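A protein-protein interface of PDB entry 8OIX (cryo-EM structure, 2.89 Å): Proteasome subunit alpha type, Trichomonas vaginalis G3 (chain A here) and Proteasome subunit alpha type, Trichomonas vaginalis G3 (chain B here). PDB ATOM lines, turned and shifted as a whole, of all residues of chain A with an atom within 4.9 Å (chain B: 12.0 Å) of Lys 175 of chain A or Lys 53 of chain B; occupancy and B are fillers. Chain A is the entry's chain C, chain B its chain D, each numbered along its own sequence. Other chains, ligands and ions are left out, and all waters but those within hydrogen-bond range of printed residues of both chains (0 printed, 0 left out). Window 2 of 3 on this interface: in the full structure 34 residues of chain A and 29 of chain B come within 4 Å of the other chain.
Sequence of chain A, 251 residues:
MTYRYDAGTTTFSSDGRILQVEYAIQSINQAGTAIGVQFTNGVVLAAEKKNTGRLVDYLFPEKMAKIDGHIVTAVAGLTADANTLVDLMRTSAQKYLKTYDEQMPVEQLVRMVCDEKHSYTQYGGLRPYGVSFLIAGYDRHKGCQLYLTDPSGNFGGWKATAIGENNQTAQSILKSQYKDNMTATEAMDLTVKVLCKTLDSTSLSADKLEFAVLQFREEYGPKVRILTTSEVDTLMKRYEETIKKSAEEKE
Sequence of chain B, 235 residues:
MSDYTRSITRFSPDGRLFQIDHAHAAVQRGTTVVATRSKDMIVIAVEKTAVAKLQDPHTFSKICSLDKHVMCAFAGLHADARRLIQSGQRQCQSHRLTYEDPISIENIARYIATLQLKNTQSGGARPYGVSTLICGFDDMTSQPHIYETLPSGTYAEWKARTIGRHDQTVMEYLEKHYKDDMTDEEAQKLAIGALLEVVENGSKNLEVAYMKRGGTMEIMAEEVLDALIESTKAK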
ATOM      1  N   LYS A 159      10.813 -24.019  30.421  1.00  0.00           N
ATOM      2  CA  LYS A 159      10.463 -24.020  31.836  1.00  0.00           C
ATOM      3  C   LYS A 159      11.377 -24.959  32.609  1.00  0.00           C
ATOM      4  O   LYS A 159      11.868 -24.618  33.691  1.00  0.00           O
ATOM      5  CB  LYS A 159       9.002 -24.425  32.024  1.00  0.00           C
ATOM      6  CG  LYS A 159       7.988 -23.421  31.511  1.00  0.00           C
ATOM      7  CD  LYS A 159       6.576 -23.942  31.716  1.00  0.00           C
ATOM      8  CE  LYS A 159       5.535 -22.929  31.277  1.00  0.00           C
ATOM      9  NZ  LYS A 159       4.153 -23.412  31.553  1.00  0.00           N
ATOM     10  N   GLN A 171      14.190 -35.300  30.660  1.00  0.00           N
ATOM     11  CA  GLN A 171      13.081 -34.490  30.169  1.00  0.00           C
ATOM     12  C   GLN A 171      11.742 -35.131  30.508  1.00  0.00           C
ATOM     13  O   GLN A 171      10.802 -34.441  30.915  1.00  0.00           O
ATOM     14  CB  GLN A 171      13.208 -34.277  28.660  1.00  0.00           C
ATOM     15  CG  GLN A 171      14.223 -33.219  28.263  1.00  0.00           C
ATOM     16  CD  GLN A 171      14.298 -33.021  26.763  1.00  0.00           C
ATOM     17  OE1 GLN A 171      13.490 -33.567  26.012  1.00  0.00           O
ATOM     18  NE2 GLN A 171      15.272 -32.235  26.318  1.00  0.00           N
ATOM     19  N   SER A 172      11.634 -36.451  30.339  1.00  0.00           N
ATOM     20  CA  SER A 172      10.396 -37.140  30.688  1.00  0.00           C
ATOM     21  C   SER A 172      10.108 -37.042  32.182  1.00  0.00           C
ATOM     22  O   SER A 172       8.958 -36.830  32.588  1.00  0.00           O
ATOM     23  CB  SER A 172      10.470 -38.604  30.252  1.00  0.00           C
ATOM     24  OG  SER A 172      11.641 -39.223  30.750  1.00  0.00           O
ATOM     25  N   ILE A 173      11.140 -37.196  33.015  1.00  0.00           N
ATOM     26  CA  ILE A 173      10.944 -37.096  34.460  1.00  0.00           C
ATOM     27  C   ILE A 173      10.490 -35.693  34.840  1.00  0.00           C
ATOM     28  O   ILE A 173       9.587 -35.520  35.667  1.00  0.00           O
ATOM     29  CB  ILE A 173      12.224 -37.504  35.209  1.00  0.00           C
ATOM     30  CG1 ILE A 173      12.554 -38.969  34.934  1.00  0.00           C
ATOM     31  CG2 ILE A 173      12.051 -37.295  36.702  1.00  0.00           C
ATOM     32  CD1 ILE A 173      13.985 -39.334  35.228  1.00  0.00           C
ATOM     33  N   LEU A 174      11.107 -34.669  34.244  1.00  0.00           N
ATOM     34  CA  LEU A 174      10.671 -33.299  34.493  1.00  0.00           C
ATOM     35  C   LEU A 174       9.226 -33.102  34.059  1.00  0.00           C
ATOM     36  O   LEU A 174       8.413 -32.555  34.809  1.00  0.00           O
ATOM     37  CB  LEU A 174      11.589 -32.311  33.772  1.00  0.00           C
ATOM     38  CG  LEU A 174      13.030 -32.189  34.264  1.00  0.00           C
ATOM     39  CD1 LEU A 174      13.854 -31.362  33.296  1.00  0.00           C
ATOM     40  CD2 LEU A 174      13.055 -31.567  35.646  1.00  0.00           C
ATOM     41  N   LYS A 175       8.874 -33.591  32.867  1.00  0.00           N
ATOM     42  CA  LYS A 175       7.508 -33.432  32.381  1.00  0.00           C
ATOM     43  C   LYS A 175       6.515 -34.068  33.340  1.00  0.00           C
ATOM     44  O   LYS A 175       5.453 -33.498  33.619  1.00  0.00           O
ATOM     45  CB  LYS A 175       7.372 -34.040  30.984  1.00  0.00           C
ATOM     46  CG  LYS A 175       5.941 -34.358  30.584  1.00  0.00           C
ATOM     47  CD  LYS A 175       5.835 -34.691  29.107  1.00  0.00           C
ATOM     48  CE  LYS A 175       4.523 -35.395  28.800  1.00  0.00           C
ATOM     49  NZ  LYS A 175       3.348 -34.604  29.257  1.00  0.00           N
ATOM     50  N   SER A 176       6.846 -35.247  33.863  1.00  0.00           N
ATOM     51  CA  SER A 176       5.955 -35.900  34.812  1.00  0.00           C
ATOM     52  C   SER A 176       5.907 -35.162  36.146  1.00  0.00           C
ATOM     53  O   SER A 176       4.869 -35.174  36.818  1.00  0.00           O
ATOM     54  CB  SER A 176       6.384 -37.351  35.025  1.00  0.00           C
ATOM     55  OG  SER A 176       5.388 -38.078  35.724  1.00  0.00           O
ATOM     56  N   GLN A 177       7.006 -34.512  36.548  1.00  0.00           N
ATOM     57  CA  GLN A 177       7.099 -33.934  37.883  1.00  0.00           C
ATOM     58  C   GLN A 177       7.132 -32.410  37.940  1.00  0.00           C
ATOM     59  O   GLN A 177       6.890 -31.855  39.015  1.00  0.00           O
ATOM     60  CB  GLN A 177       8.345 -34.469  38.604  1.00  0.00           C
ATOM     61  CG  GLN A 177       8.180 -35.852  39.205  1.00  0.00           C
ATOM     62  CD  GLN A 177       8.999 -36.033  40.469  1.00  0.00           C
ATOM     63  OE1 GLN A 177       9.305 -35.067  41.167  1.00  0.00           O
ATOM     64  NE2 GLN A 177       9.358 -37.276  40.771  1.00  0.00           N
ATOM     65  N   TYR A 178       7.427 -31.719  36.839  1.00  0.00           N
ATOM     66  CA  TYR A 178       7.615 -30.273  36.911  1.00  0.00           C
ATOM     67  C   TYR A 178       6.293 -29.560  37.160  1.00  0.00           C
ATOM     68  O   TYR A 178       5.288 -29.835  36.499  1.00  0.00           O
ATOM     69  CB  TYR A 178       8.256 -29.738  35.631  1.00  0.00           C
ATOM     70  CG  TYR A 178       8.354 -28.230  35.572  1.00  0.00           C
ATOM     71  CD1 TYR A 178       9.332 -27.549  36.285  1.00  0.00           C
ATOM     72  CD2 TYR A 178       7.473 -27.488  34.798  1.00  0.00           C
ATOM     73  CE1 TYR A 178       9.425 -26.171  36.232  1.00  0.00           C
ATOM     74  CE2 TYR A 178       7.557 -26.112  34.738  1.00  0.00           C
ATOM     75  CZ  TYR A 178       8.535 -25.459  35.456  1.00  0.00           C
ATOM     76  OH  TYR A 178       8.622 -24.087  35.398  1.00  0.00           O
ATOM     77  N   LYS B  48       3.690 -24.681  15.466  1.00  0.00           N
ATOM     78  CA  LYS B  48       4.751 -24.770  16.461  1.00  0.00           C
ATOM     79  C   LYS B  48       4.787 -26.158  17.081  1.00  0.00           C
ATOM     80  O   LYS B  48       3.775 -26.635  17.607  1.00  0.00           O
ATOM     81  CB  LYS B  48       4.567 -23.719  17.558  1.00  0.00           C
ATOM     82  CG  LYS B  48       4.485 -22.292  17.053  1.00  0.00           C
ATOM     83  CD  LYS B  48       4.676 -21.305  18.189  1.00  0.00           C
ATOM     84  CE  LYS B  48       3.666 -21.540  19.299  1.00  0.00           C
ATOM     85  NZ  LYS B  48       2.270 -21.342  18.829  1.00  0.00           N
ATOM     86  N   THR B  49       5.950 -26.797  17.022  1.00  0.00           N
ATOM     87  CA  THR B  49       6.184 -28.074  17.685  1.00  0.00           C
ATOM     88  C   THR B  49       6.972 -27.814  18.967  1.00  0.00           C
ATOM     89  O   THR B  49       8.074 -27.257  18.925  1.00  0.00           O
ATOM     90  CB  THR B  49       6.906 -29.057  16.758  1.00  0.00           C
ATOM     91  OG1 THR B  49       7.125 -30.299  17.441  1.00  0.00           O
ATOM     92  CG2 THR B  49       8.230 -28.495  16.233  1.00  0.00           C
ATOM     93  N   ALA B  50       6.389 -28.179  20.106  1.00  0.00           N
ATOM     94  CA  ALA B  50       6.998 -27.850  21.385  1.00  0.00           C
ATOM     95  C   ALA B  50       6.449 -28.766  22.467  1.00  0.00           C
ATOM     96  O   ALA B  50       5.416 -29.418  22.293  1.00  0.00           O
ATOM     97  CB  ALA B  50       6.761 -26.381  21.756  1.00  0.00           C
ATOM     98  N   VAL B  51       7.162 -28.803  23.592  1.00  0.00           N
ATOM     99  CA  VAL B  51       6.719 -29.512  24.791  1.00  0.00           C
ATOM    100  C   VAL B  51       5.991 -28.505  25.671  1.00  0.00           C
ATOM    101  O   VAL B  51       6.602 -27.767  26.447  1.00  0.00           O
ATOM    102  CB  VAL B  51       7.898 -30.153  25.512  1.00  0.00           C
ATOM    103  N   ALA B  52       4.662 -28.474  25.538  1.00  0.00           N
ATOM    104  CA  ALA B  52       3.861 -27.418  26.152  1.00  0.00           C
ATOM    105  C   ALA B  52       4.056 -27.340  27.661  1.00  0.00           C
ATOM    106  O   ALA B  52       3.951 -26.252  28.241  1.00  0.00           O
ATOM    107  CB  ALA B  52       2.383 -27.627  25.822  1.00  0.00           C
ATOM    108  N   LYS B  53       4.336 -28.467  28.314  1.00  0.00           N
ATOM    109  CA  LYS B  53       4.455 -28.470  29.766  1.00  0.00           C
ATOM    110  C   LYS B  53       5.846 -28.072  30.255  1.00  0.00           C
ATOM    111  O   LYS B  53       6.014 -27.818  31.453  1.00  0.00           O
ATOM    112  CB  LYS B  53       4.076 -29.852  30.313  1.00  0.00           C
ATOM    113  CG  LYS B  53       3.909 -29.914  31.826  1.00  0.00           C
ATOM    114  CD  LYS B  53       3.299 -31.227  32.281  1.00  0.00           C
ATOM    115  CE  LYS B  53       3.160 -31.262  33.795  1.00  0.00           C
ATOM    116  NZ  LYS B  53       2.565 -32.538  34.276  1.00  0.00           N
ATOM    117  N   LEU B  54       6.839 -27.976  29.368  1.00  0.00           N
ATOM    118  CA  LEU B  54       8.213 -27.786  29.808  1.00  0.00           C
ATOM    119  C   LEU B  54       8.968 -26.669  29.102  1.00  0.00           C
ATOM    120  O   LEU B  54      10.150 -26.471  29.403  1.00  0.00           O
ATOM    121  CB  LEU B  54       9.011 -29.089  29.642  1.00  0.00           C
ATOM    122  CG  LEU B  54       8.851 -30.143  30.735  1.00  0.00           C
ATOM    123  CD1 LEU B  54       9.789 -31.309  30.477  1.00  0.00           C
ATOM    124  CD2 LEU B  54       9.113 -29.534  32.099  1.00  0.00           C
ATOM    125  N   GLN B  55       8.343 -25.930  28.190  1.00  0.00           N
ATOM    126  CA  GLN B  55       9.057 -24.853  27.521  1.00  0.00           C
ATOM    127  C   GLN B  55       8.113 -23.699  27.227  1.00  0.00           C
ATOM    128  O   GLN B  55       6.893 -23.864  27.153  1.00  0.00           O
ATOM    129  CB  GLN B  55       9.740 -25.338  26.236  1.00  0.00           C
ATOM    130  CG  GLN B  55       8.806 -25.651  25.090  1.00  0.00           C
ATOM    131  CD  GLN B  55       9.559 -26.129  23.865  1.00  0.00           C
ATOM    132  OE1 GLN B  55       9.388 -27.261  23.418  1.00  0.00           O
ATOM    133  NE2 GLN B  55      10.403 -25.264  23.316  1.00  0.00           N
ATOM    134  N   ASP B  56       8.705 -22.520  27.065  1.00  0.00           N
ATOM    135  CA  ASP B  56       7.955 -21.305  26.776  1.00  0.00           C
ATOM    136  C   ASP B  56       7.671 -21.211  25.280  1.00  0.00           C
ATOM    137  O   ASP B  56       8.604 -21.278  24.475  1.00  0.00           O
ATOM    138  CB  ASP B  56       8.728 -20.076  27.239  1.00  0.00           C
ATOM    139  CG  ASP B  56       8.984 -20.079  28.732  1.00  0.00           C
ATOM    140  OD1 ASP B  56       8.225 -20.747  29.467  1.00  0.00           O
ATOM    141  OD2 ASP B  56       9.944 -19.414  29.172  1.00  0.00           O
ATOM    142  N   PRO B  57       6.410 -21.056  24.875  1.00  0.00           N
ATOM    143  CA  PRO B  57       6.100 -20.946  23.442  1.00  0.00           C
ATOM    144  C   PRO B  57       6.394 -19.567  22.868  1.00  0.00           C
ATOM    145  O   PRO B  57       5.929 -19.237  21.773  1.00  0.00           O
ATOM    146  CB  PRO B  57       4.597 -21.263  23.379  1.00  0.00           C
ATOM    147  CG  PRO B  57       4.222 -21.772  24.751  1.00  0.00           C
ATOM    148  CD  PRO B  57       5.195 -21.156  25.696  1.00  0.00           C
ATOM    149  N   HIS B  58       7.163 -18.753  23.592  1.00  0.00           N
ATOM    150  CA  HIS B  58       7.435 -17.383  23.177  1.00  0.00           C
ATOM    151  C   HIS B  58       8.548 -17.275  22.140  1.00  0.00           C
ATOM    152  O   HIS B  58       8.817 -16.168  21.663  1.00  0.00           O
ATOM    153  CB  HIS B  58       7.779 -16.521  24.394  1.00  0.00           C
ATOM    154  CG  HIS B  58       6.596 -15.823  24.989  1.00  0.00           C
ATOM    155  ND1 HIS B  58       5.643 -16.478  25.741  1.00  0.00           N
ATOM    156  CD2 HIS B  58       6.210 -14.526  24.941  1.00  0.00           C
ATOM    157  CE1 HIS B  58       4.723 -15.614  26.129  1.00  0.00           C
ATOM    158  NE2 HIS B  58       5.043 -14.422  25.658  1.00  0.00           N
ATOM    159  N   ASN B 201      -3.972 -29.711  16.159  1.00  0.00           N
ATOM    160  CA  ASN B 201      -4.079 -28.992  17.420  1.00  0.00           C
ATOM    161  C   ASN B 201      -4.525 -27.562  17.152  1.00  0.00           C
ATOM    162  O   ASN B 201      -4.316 -27.021  16.063  1.00  0.00           O
ATOM    163  CB  ASN B 201      -2.751 -28.996  18.188  1.00  0.00           C
ATOM    164  CG  ASN B 201      -2.389 -30.367  18.720  1.00  0.00           C
ATOM    165  OD1 ASN B 201      -2.943 -30.823  19.720  1.00  0.00           O
ATOM    166  ND2 ASN B 201      -1.453 -31.032  18.055  1.00  0.00           N
ATOM    167  N   LYS B 204      -3.244 -23.815  21.021  1.00  0.00           N
ATOM    168  CA  LYS B 204      -2.075 -24.196  21.806  1.00  0.00           C
ATOM    169  C   LYS B 204      -0.867 -24.510  20.933  1.00  0.00           C
ATOM    170  O   LYS B 204       0.265 -24.484  21.430  1.00  0.00           O
ATOM    171  CB  LYS B 204      -2.405 -25.398  22.692  1.00  0.00           C
ATOM    172  CG  LYS B 204      -2.941 -26.603  21.937  1.00  0.00           C
ATOM    173  CD  LYS B 204      -3.285 -27.738  22.888  1.00  0.00           C
ATOM    174  CE  LYS B 204      -4.494 -27.399  23.745  1.00  0.00           C
ATOM    175  NZ  LYS B 204      -5.710 -27.150  22.924  1.00  0.00           N
ATOM    176  N   ASN B 205      -1.076 -24.803  19.652  1.00  0.00           N
ATOM    177  CA  ASN B 205       0.002 -25.112  18.722  1.00  0.00           C
ATOM    178  C   ASN B 205       0.274 -23.979  17.744  1.00  0.00           C
ATOM    179  O   ASN B 205       1.419 -23.539  17.611  1.00  0.00           O
ATOM    180  CB  ASN B 205      -0.327 -26.406  17.956  1.00  0.00           C
ATOM    181  CG  ASN B 205       0.685 -26.724  16.867  1.00  0.00           C
ATOM    182  OD1 ASN B 205       0.717 -26.081  15.817  1.00  0.00           O
ATOM    183  ND2 ASN B 205       1.520 -27.726  17.115  1.00  0.00           N
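N of Val 51 of chain B is in hydrogen-bond range of OE1 of Gln 55 of chain B (2.7 Å).
Of chain B, only Lys 53 and Leu 54 come within 4 Å of Lys 175 of chain A.
Printed residues of chain A within 4 Å of Lys 53 of chain B: Lys 159 (3.9 Å), Lys 175 (3.1 Å) and Tyr 178 (3.7 Å).
Lys 159 of chain A touches four residues of chain B.
Leu 174 of chain A touches just one residue of chain B: Leu 54 (3.9 Å).
No residue of chain B comes within 4 Å of Ser 176 of chain A.
Printed residues of chain B within 4 Å of Tyr 178 of chain A: Lys 53 (3.7 Å) and Leu 54 (3.6 Å).
Printed residues of chain B within 4 Å of Gln 171 of chain A: Leu 54.
Of the printed residues of chain A, Gln 55 of chain B touches Lys 159.
Of the printed residues of chain A, Asp 56 of chain B touches Lys 159 (3.4 Å).
Of the printed residues of chain A, Leu 54 of chain B touches Lys 159, Gln 171, Leu 174, Lys 175 and Tyr 178.
Ile 173 of chain A touches none of the printed residues of chain B.
Ala 52 of chain B touches none of the printed residues of chain A.
The nearest residue of chain B that does not touch Lys 175 of chain A is Val 51 of chain B (6.1 Å).
The nearest printed residue of chain B that does not touch Gln 171 of chain A is Val 51 of chain B (6.6 Å).
O of Leu 54 of chain B is in hydrogen-bond range of N of Lys 159 of chain A, 2.7 Å away.
The backbone carbonyl oxygen (O) of Lys 175 of chain A lies within hydrogen-bond range of the side-chain amino group (NZ) of Lys 53 of chain B, 3.1 Å away.
O of Lys 53 of chain B touches CD of Lys 159 of chain A, 3.9 Å away.
Lys 159 of chain A touches Gln 55 of chain B.
Lys 159 of chain A touches Asp 56 of chain B.
Gln 171 of chain A touches Leu 54 of chain B (O to CD1, 3.3 Å).
Leu 54 of chain B touches Leu 174 of chain A.
Lys 175 of chain A touches Leu 54 of chain B (N to CD1, 3.4 Å).
O of Lys 53 of chain B touches CD2 of Tyr 178 of chain A, 3.7 Å away.
CB of Tyr 178 of chain A touches CD2 of Leu 54 of chain B, at 3.6 Å.
Printed residues of chain A that touch a printed residue of chain B: Lys 159, Gln 171, Leu 174, Lys 175 and Tyr 178.
Hydrophobic or aromatic side chains of chain A that line the printed part of chain B: Leu 174 and Tyr 178.
Among the printed residues, 10 pairs touch across the chains.
Among the printed residues, no Asp or Glu carboxylate lies within 4 Å of a Lys or Arg side-chain nitrogen of the other chain.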
